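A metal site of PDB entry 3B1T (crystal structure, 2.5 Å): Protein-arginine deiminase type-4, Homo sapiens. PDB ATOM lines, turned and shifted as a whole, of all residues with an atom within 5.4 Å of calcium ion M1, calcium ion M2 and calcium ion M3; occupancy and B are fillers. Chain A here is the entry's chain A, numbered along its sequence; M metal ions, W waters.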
ATOM      1  N   ASN A 161     -18.616  -4.306 -13.385  1.00  0.00           N
ATOM      2  CA  ASN A 161     -18.204  -4.921 -12.143  1.00  0.00           C
ATOM      3  C   ASN A 161     -16.682  -4.931 -12.049  1.00  0.00           C
ATOM      4  O   ASN A 161     -16.010  -5.968 -12.028  1.00  0.00           O
ATOM      5  CB  ASN A 161     -18.820  -6.318 -12.067  1.00  0.00           C
ATOM      6  CG  ASN A 161     -18.615  -7.004 -10.723  1.00  0.00           C
ATOM      7  OD1 ASN A 161     -18.450  -6.368  -9.641  1.00  0.00           O
ATOM      8  ND2 ASN A 161     -18.625  -8.318 -10.777  1.00  0.00           N
ATOM      9  N   ASP A 163     -14.695  -3.472  -9.732  1.00  0.00           N
ATOM     10  CA  ASP A 163     -14.045  -3.396  -8.423  1.00  0.00           C
ATOM     11  C   ASP A 163     -13.456  -4.769  -8.061  1.00  0.00           C
ATOM     12  O   ASP A 163     -13.508  -5.696  -8.881  1.00  0.00           O
ATOM     13  CB  ASP A 163     -15.031  -2.884  -7.361  1.00  0.00           C
ATOM     14  CG  ASP A 163     -16.013  -3.950  -6.887  1.00  0.00           C
ATOM     15  OD1 ASP A 163     -16.412  -4.818  -7.703  1.00  0.00           O
ATOM     16  OD2 ASP A 163     -16.388  -3.925  -5.695  1.00  0.00           O
ATOM     17  N   ARG A 164     -12.888  -4.870  -6.854  1.00  0.00           N
ATOM     18  CA  ARG A 164     -12.223  -6.097  -6.388  1.00  0.00           C
ATOM     19  C   ARG A 164     -12.659  -6.496  -4.958  1.00  0.00           C
ATOM     20  O   ARG A 164     -11.952  -6.220  -3.982  1.00  0.00           O
ATOM     21  CB  ARG A 164     -10.694  -5.936  -6.463  1.00  0.00           C
ATOM     22  CG  ARG A 164      -9.907  -7.219  -6.193  1.00  0.00           C
ATOM     23  CD  ARG A 164      -8.404  -7.032  -6.376  1.00  0.00           C
ATOM     24  NE  ARG A 164      -7.725  -6.674  -5.111  1.00  0.00           N
ATOM     25  CZ  ARG A 164      -6.990  -5.581  -4.906  1.00  0.00           C
ATOM     26  NH1 ARG A 164      -6.788  -4.663  -5.867  1.00  0.00           N
ATOM     27  NH2 ARG A 164      -6.427  -5.385  -3.706  1.00  0.00           N
ATOM     28  N   ASP A 165     -13.812  -7.159  -4.870  1.00  0.00           N
ATOM     29  CA  ASP A 165     -14.341  -7.678  -3.603  1.00  0.00           C
ATOM     30  C   ASP A 165     -13.628  -8.987  -3.175  1.00  0.00           C
ATOM     31  O   ASP A 165     -13.805  -9.445  -2.038  1.00  0.00           O
ATOM     32  CB  ASP A 165     -15.864  -7.915  -3.690  1.00  0.00           C
ATOM     33  CG  ASP A 165     -16.663  -6.641  -3.998  1.00  0.00           C
ATOM     34  OD1 ASP A 165     -16.582  -5.656  -3.226  1.00  0.00           O
ATOM     35  OD2 ASP A 165     -17.399  -6.611  -5.019  1.00  0.00           O
ATOM     36  N   ASP A 173     -13.057  -8.257 -10.518  1.00  0.00           N
ATOM     37  CA  ASP A 173     -14.066  -9.337 -10.416  1.00  0.00           C
ATOM     38  C   ASP A 173     -14.540  -9.887 -11.797  1.00  0.00           C
ATOM     39  O   ASP A 173     -14.662 -11.101 -11.964  1.00  0.00           O
ATOM     40  CB  ASP A 173     -15.288  -8.860  -9.613  1.00  0.00           C
ATOM     41  CG  ASP A 173     -14.986  -8.547  -8.141  1.00  0.00           C
ATOM     42  OD1 ASP A 173     -13.944  -9.001  -7.596  1.00  0.00           O
ATOM     43  OD2 ASP A 173     -15.799  -7.837  -7.504  1.00  0.00           O
ATOM     44  N   CYS A 174     -14.806  -8.989 -12.759  1.00  0.00           N
ATOM     45  CA  CYS A 174     -15.381  -9.337 -14.085  1.00  0.00           C
ATOM     46  C   CYS A 174     -14.426  -9.958 -15.128  1.00  0.00           C
ATOM     47  O   CYS A 174     -14.852 -10.364 -16.217  1.00  0.00           O
ATOM     48  CB  CYS A 174     -16.085  -8.109 -14.706  1.00  0.00           C
ATOM     49  SG  CYS A 174     -15.014  -6.684 -15.094  1.00  0.00           S
ATOM     50  N   GLU A 175     -13.135 -10.061 -14.783  1.00  0.00           N
ATOM     51  CA  GLU A 175     -12.162 -10.717 -15.667  1.00  0.00           C
ATOM     52  C   GLU A 175     -12.376 -12.236 -15.797  1.00  0.00           C
ATOM     53  O   GLU A 175     -11.792 -12.865 -16.677  1.00  0.00           O
ATOM     54  CB  GLU A 175     -10.722 -10.411 -15.209  1.00  0.00           C
ATOM     55  CG  GLU A 175     -10.332  -8.948 -15.375  1.00  0.00           C
ATOM     56  CD  GLU A 175      -8.819  -8.726 -15.429  1.00  0.00           C
ATOM     57  OE1 GLU A 175      -8.061  -9.688 -15.192  1.00  0.00           O
ATOM     58  OE2 GLU A 175      -8.399  -7.581 -15.704  1.00  0.00           O
ATOM     59  N   ASP A 176     -13.200 -12.808 -14.920  1.00  0.00           N
ATOM     60  CA  ASP A 176     -13.514 -14.243 -14.972  1.00  0.00           C
ATOM     61  C   ASP A 176     -15.035 -14.525 -14.956  1.00  0.00           C
ATOM     62  O   ASP A 176     -15.843 -13.640 -14.641  1.00  0.00           O
ATOM     63  CB  ASP A 176     -12.805 -14.985 -13.836  1.00  0.00           C
ATOM     64  CG  ASP A 176     -13.312 -14.579 -12.455  1.00  0.00           C
ATOM     65  OD1 ASP A 176     -12.521 -14.698 -11.484  1.00  0.00           O
ATOM     66  OD2 ASP A 176     -14.472 -14.142 -12.315  1.00  0.00           O
ATOM     67  N   ASP A 177     -15.371 -15.771 -15.265  1.00  0.00           N
ATOM     68  CA  ASP A 177     -16.781 -16.214 -15.398  1.00  0.00           C
ATOM     69  C   ASP A 177     -17.288 -16.923 -14.130  1.00  0.00           C
ATOM     70  O   ASP A 177     -18.010 -17.921 -14.197  1.00  0.00           O
ATOM     71  CB  ASP A 177     -16.953 -17.095 -16.655  1.00  0.00           C
ATOM     72  CG  ASP A 177     -15.792 -18.075 -16.863  1.00  0.00           C
ATOM     73  OD1 ASP A 177     -15.747 -19.113 -16.170  1.00  0.00           O
ATOM     74  OD2 ASP A 177     -14.938 -17.815 -17.727  1.00  0.00           O
ATOM     75  N   GLU A 178     -16.937 -16.355 -12.970  1.00  0.00           N
ATOM     76  CA  GLU A 178     -17.217 -16.962 -11.667  1.00  0.00           C
ATOM     77  C   GLU A 178     -17.626 -15.898 -10.629  1.00  0.00           C
ATOM     78  O   GLU A 178     -17.079 -14.787 -10.602  1.00  0.00           O
ATOM     79  CB  GLU A 178     -15.992 -17.758 -11.158  1.00  0.00           C
ATOM     80  CG  GLU A 178     -15.451 -18.837 -12.139  1.00  0.00           C
ATOM     81  CD  GLU A 178     -14.235 -19.598 -11.599  1.00  0.00           C
ATOM     82  OE1 GLU A 178     -13.710 -19.221 -10.529  1.00  0.00           O
ATOM     83  OE2 GLU A 178     -13.798 -20.576 -12.247  1.00  0.00           O
ATOM     84  N   VAL A 179     -18.602 -16.250  -9.779  1.00  0.00           N
ATOM     85  CA  VAL A 179     -18.993 -15.430  -8.636  1.00  0.00           C
ATOM     86  C   VAL A 179     -18.438 -16.107  -7.379  1.00  0.00           C
ATOM     87  O   VAL A 179     -18.947 -17.152  -6.957  1.00  0.00           O
ATOM     88  CB  VAL A 179     -20.535 -15.313  -8.484  1.00  0.00           C
ATOM     89  CG1 VAL A 179     -20.878 -14.358  -7.354  1.00  0.00           C
ATOM     90  CG2 VAL A 179     -21.157 -14.846  -9.762  1.00  0.00           C
ATOM     91  N   GLU A 183     -20.818 -11.263  -1.531  1.00  0.00           N
ATOM     92  CA  GLU A 183     -20.660  -9.813  -1.540  1.00  0.00           C
ATOM     93  C   GLU A 183     -20.657  -9.266  -2.972  1.00  0.00           C
ATOM     94  O   GLU A 183     -21.132  -8.159  -3.216  1.00  0.00           O
ATOM     95  CB  GLU A 183     -19.325  -9.411  -0.871  1.00  0.00           C
ATOM     96  CG  GLU A 183     -19.224  -9.680   0.624  1.00  0.00           C
ATOM     97  CD  GLU A 183     -18.717 -11.079   0.952  1.00  0.00           C
ATOM     98  OE1 GLU A 183     -17.902 -11.206   1.888  1.00  0.00           O
ATOM     99  OE2 GLU A 183     -19.140 -12.050   0.296  1.00  0.00           O
ATOM    100  N   ASP A 184     -20.101 -10.038  -3.894  1.00  0.00           N
ATOM    101  CA  ASP A 184     -19.996  -9.629  -5.270  1.00  0.00           C
ATOM    102  C   ASP A 184     -21.403  -9.511  -5.919  1.00  0.00           C
ATOM    103  O   ASP A 184     -21.610  -8.622  -6.779  1.00  0.00           O
ATOM    104  CB  ASP A 184     -19.075 -10.603  -6.042  1.00  0.00           C
ATOM    105  CG  ASP A 184     -18.704 -10.089  -7.442  1.00  0.00           C
ATOM    106  OD1 ASP A 184     -18.614 -10.930  -8.374  1.00  0.00           O
ATOM    107  OD2 ASP A 184     -18.506  -8.865  -7.626  1.00  0.00           O
ATOM    108  N   ASP A 187     -23.217  -6.024  -6.265  1.00  0.00           N
ATOM    109  CA  ASP A 187     -22.857  -5.104  -7.359  1.00  0.00           C
ATOM    110  C   ASP A 187     -23.660  -5.375  -8.622  1.00  0.00           C
ATOM    111  O   ASP A 187     -23.621  -4.589  -9.558  1.00  0.00           O
ATOM    112  CB  ASP A 187     -21.354  -5.212  -7.697  1.00  0.00           C
ATOM    113  CG  ASP A 187     -20.472  -4.681  -6.587  1.00  0.00           C
ATOM    114  OD1 ASP A 187     -20.781  -3.608  -6.038  1.00  0.00           O
ATOM    115  OD2 ASP A 187     -19.459  -5.340  -6.276  1.00  0.00           O
ATOM    116  N   ARG A 220     -22.153 -10.381 -18.444  1.00  0.00           N
ATOM    117  CA  ARG A 220     -22.166 -11.742 -17.936  1.00  0.00           C
ATOM    118  C   ARG A 220     -23.384 -11.962 -17.033  1.00  0.00           C
ATOM    119  O   ARG A 220     -23.786 -11.051 -16.287  1.00  0.00           O
ATOM    120  CB  ARG A 220     -20.875 -12.084 -17.198  1.00  0.00           C
ATOM    121  CG  ARG A 220     -20.776 -13.582 -16.921  1.00  0.00           C
ATOM    122  CD  ARG A 220     -19.530 -13.954 -16.254  1.00  0.00           C
ATOM    123  NE  ARG A 220     -18.379 -13.844 -17.142  1.00  0.00           N
ATOM    124  CZ  ARG A 220     -17.443 -12.914 -17.042  1.00  0.00           C
ATOM    125  NH1 ARG A 220     -17.499 -11.985 -16.099  1.00  0.00           N
ATOM    126  NH2 ARG A 220     -16.425 -12.907 -17.901  1.00  0.00           N
ATOM    127  N   PHE A 222     -25.436 -14.671 -14.412  1.00  0.00           N
ATOM    128  CA  PHE A 222     -25.391 -15.879 -13.583  1.00  0.00           C
ATOM    129  C   PHE A 222     -26.787 -16.291 -13.129  1.00  0.00           C
ATOM    130  O   PHE A 222     -27.588 -15.436 -12.743  1.00  0.00           O
ATOM    131  CB  PHE A 222     -24.535 -15.653 -12.328  1.00  0.00           C
ATOM    132  CG  PHE A 222     -23.183 -15.079 -12.595  1.00  0.00           C
ATOM    133  CD1 PHE A 222     -23.009 -13.711 -12.696  1.00  0.00           C
ATOM    134  CD2 PHE A 222     -22.066 -15.889 -12.716  1.00  0.00           C
ATOM    135  CE1 PHE A 222     -21.749 -13.173 -12.944  1.00  0.00           C
ATOM    136  CE2 PHE A 222     -20.802 -15.350 -12.945  1.00  0.00           C
ATOM    137  CZ  PHE A 222     -20.641 -13.999 -13.054  1.00  0.00           C
ATOM    138  N   GLU A 260     -23.965  -8.544 -14.610  1.00  0.00           N
ATOM    139  CA  GLU A 260     -22.864  -7.562 -14.513  1.00  0.00           C
ATOM    140  C   GLU A 260     -22.427  -7.157 -15.892  1.00  0.00           C
ATOM    141  O   GLU A 260     -22.584  -7.917 -16.819  1.00  0.00           O
ATOM    142  CB  GLU A 260     -21.635  -8.142 -13.807  1.00  0.00           C
ATOM    143  CG  GLU A 260     -21.127  -9.429 -14.491  1.00  0.00           C
ATOM    144  CD  GLU A 260     -19.910 -10.003 -13.875  1.00  0.00           C
ATOM    145  OE1 GLU A 260     -19.561  -9.638 -12.740  1.00  0.00           O
ATOM    146  OE2 GLU A 260     -19.269 -10.826 -14.547  1.00  0.00           O
ATOM    147  N   LYS A 370     -26.962   0.140  -6.028  1.00  0.00           N
ATOM    148  CA  LYS A 370     -25.580   0.208  -5.583  1.00  0.00           C
ATOM    149  C   LYS A 370     -24.773   1.374  -6.189  1.00  0.00           C
ATOM    150  O   LYS A 370     -24.724   1.544  -7.415  1.00  0.00           O
ATOM    151  CB  LYS A 370     -24.887  -1.115  -5.905  1.00  0.00           C
ATOM    152  CG  LYS A 370     -23.405  -1.132  -5.538  1.00  0.00           C
ATOM    153  CD  LYS A 370     -23.152  -0.801  -4.068  1.00  0.00           C
ATOM    154  CE  LYS A 370     -22.578  -1.974  -3.291  1.00  0.00           C
ATOM    155  NZ  LYS A 370     -21.744  -1.455  -2.141  1.00  0.00           N
ATOM    156  N   LEU A 372     -20.869   2.982  -6.141  1.00  0.00           N
ATOM    157  CA  LEU A 372     -19.516   2.739  -5.682  1.00  0.00           C
ATOM    158  C   LEU A 372     -18.532   3.634  -6.345  1.00  0.00           C
ATOM    159  O   LEU A 372     -18.755   4.030  -7.484  1.00  0.00           O
ATOM    160  CB  LEU A 372     -19.105   1.276  -5.874  1.00  0.00           C
ATOM    161  CG  LEU A 372     -18.906   0.612  -7.239  1.00  0.00           C
ATOM    162  CD1 LEU A 372     -17.479   0.047  -7.376  1.00  0.00           C
ATOM    163  CD2 LEU A 372     -19.923  -0.509  -7.450  1.00  0.00           C
ATOM    164  N   PRO A 395     -12.212  -3.470  -2.356  1.00  0.00           N
ATOM    165  CA  PRO A 395     -13.588  -3.711  -1.932  1.00  0.00           C
ATOM    166  C   PRO A 395     -14.414  -2.441  -1.970  1.00  0.00           C
ATOM    167  O   PRO A 395     -14.141  -1.484  -1.234  1.00  0.00           O
ATOM    168  CB  PRO A 395     -13.444  -4.253  -0.508  1.00  0.00           C
ATOM    169  CG  PRO A 395     -12.046  -4.755  -0.417  1.00  0.00           C
ATOM    170  CD  PRO A 395     -11.249  -3.848  -1.299  1.00  0.00           C
ATOM    171  N   ASP A 396     -15.428  -2.454  -2.844  1.00  0.00           N
ATOM    172  CA  ASP A 396     -16.208  -1.284  -3.214  1.00  0.00           C
ATOM    173  C   ASP A 396     -15.333  -0.119  -3.701  1.00  0.00           C
ATOM    174  O   ASP A 396     -15.513   1.030  -3.310  1.00  0.00           O
ATOM    175  CB  ASP A 396     -17.179  -0.893  -2.101  1.00  0.00           C
ATOM    176  CG  ASP A 396     -18.361  -1.853  -1.989  1.00  0.00           C
ATOM    177  OD1 ASP A 396     -18.484  -2.789  -2.836  1.00  0.00           O
ATOM    178  OD2 ASP A 396     -19.176  -1.678  -1.052  1.00  0.00           O
HETATM  179 CA    CA M   1     -16.180 -12.770 -11.391  1.00  0.00          CA
HETATM  180 CA    CA M   2     -17.820  -6.654  -7.330  1.00  0.00          CA
HETATM  181 CA    CA M   3     -18.290  -4.452  -4.427  1.00  0.00          CA
HETATM  182  O   HOH W   1     -20.135  -5.686  -3.059  1.00  0.00           O
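OD2 of Asp 396 lies within salt-bridge range of NZ of Lys 370, at 2.8 Å.
The backbone carbonyl oxygen (O) of Asp 176 lies within hydrogen-bond range of the guanidinium group (NH1) of Arg 220 (2.8 Å).
The backbone carbonyl oxygen (O) of Asn 161 lies within hydrogen-bond range of the side-chain sulfur (SG) of Cys 174, 3.3 Å away.
ND2 of Asn 161 is in hydrogen-bond range of OE1 of Glu 260 (2.5 Å).
Within 4 Å of calcium ion M1: Asp 173, Asp 176 and Glu 178.
The nearest printed residue that does not touch calcium ion M1 is Cys 174 (4.2 Å).
Along chain A the residues within 4 Å of calcium ion M2 span positions 161 to 187.
Four residues have an atom within 4 Å of calcium ion M3: Asp 163, Asp 165, Asp 187 and Asp 396.
Calcium ion M1 is bound by O of Asp 173 (2.3 Å), O of Glu 178 (2.3 Å) and OD2 of Asp 176 (2.4 Å).
Calcium ion M2 is bound by OD2 of Asp 184 (2.3 Å), OD1 of Asp 163 (2.3 Å), OD2 of Asp 173 (2.3 Å), OD2 of Asp 187 (2.4 Å), OD2 of Asp 165 (2.3 Å) and OD1 of Asn 161 (2.4 Å).
OD1 of Asp 396 is bound to calcium ion M3, at 2.3 Å.
OD2 of Asp 163 binds calcium ion M3 (2.3 Å).
Calcium ion M3 is bound by OD2 of Asp 187, 2.4 Å away.
OD2 of Asp 165 is bound to calcium ion M3, at 2.4 Å.
The side-chain carboxylate (OD1) of Asp 165 binds calcium ion M3, at 2.4 Å.
Water W1 is bound to calcium ion M3 (2.6 Å).
Calcium ion M3 has six donor atoms within binding distance.
Slightly farther from calcium ion M3 lies the side-chain carboxylate (OD1) of Asp 187 (3.1 Å).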
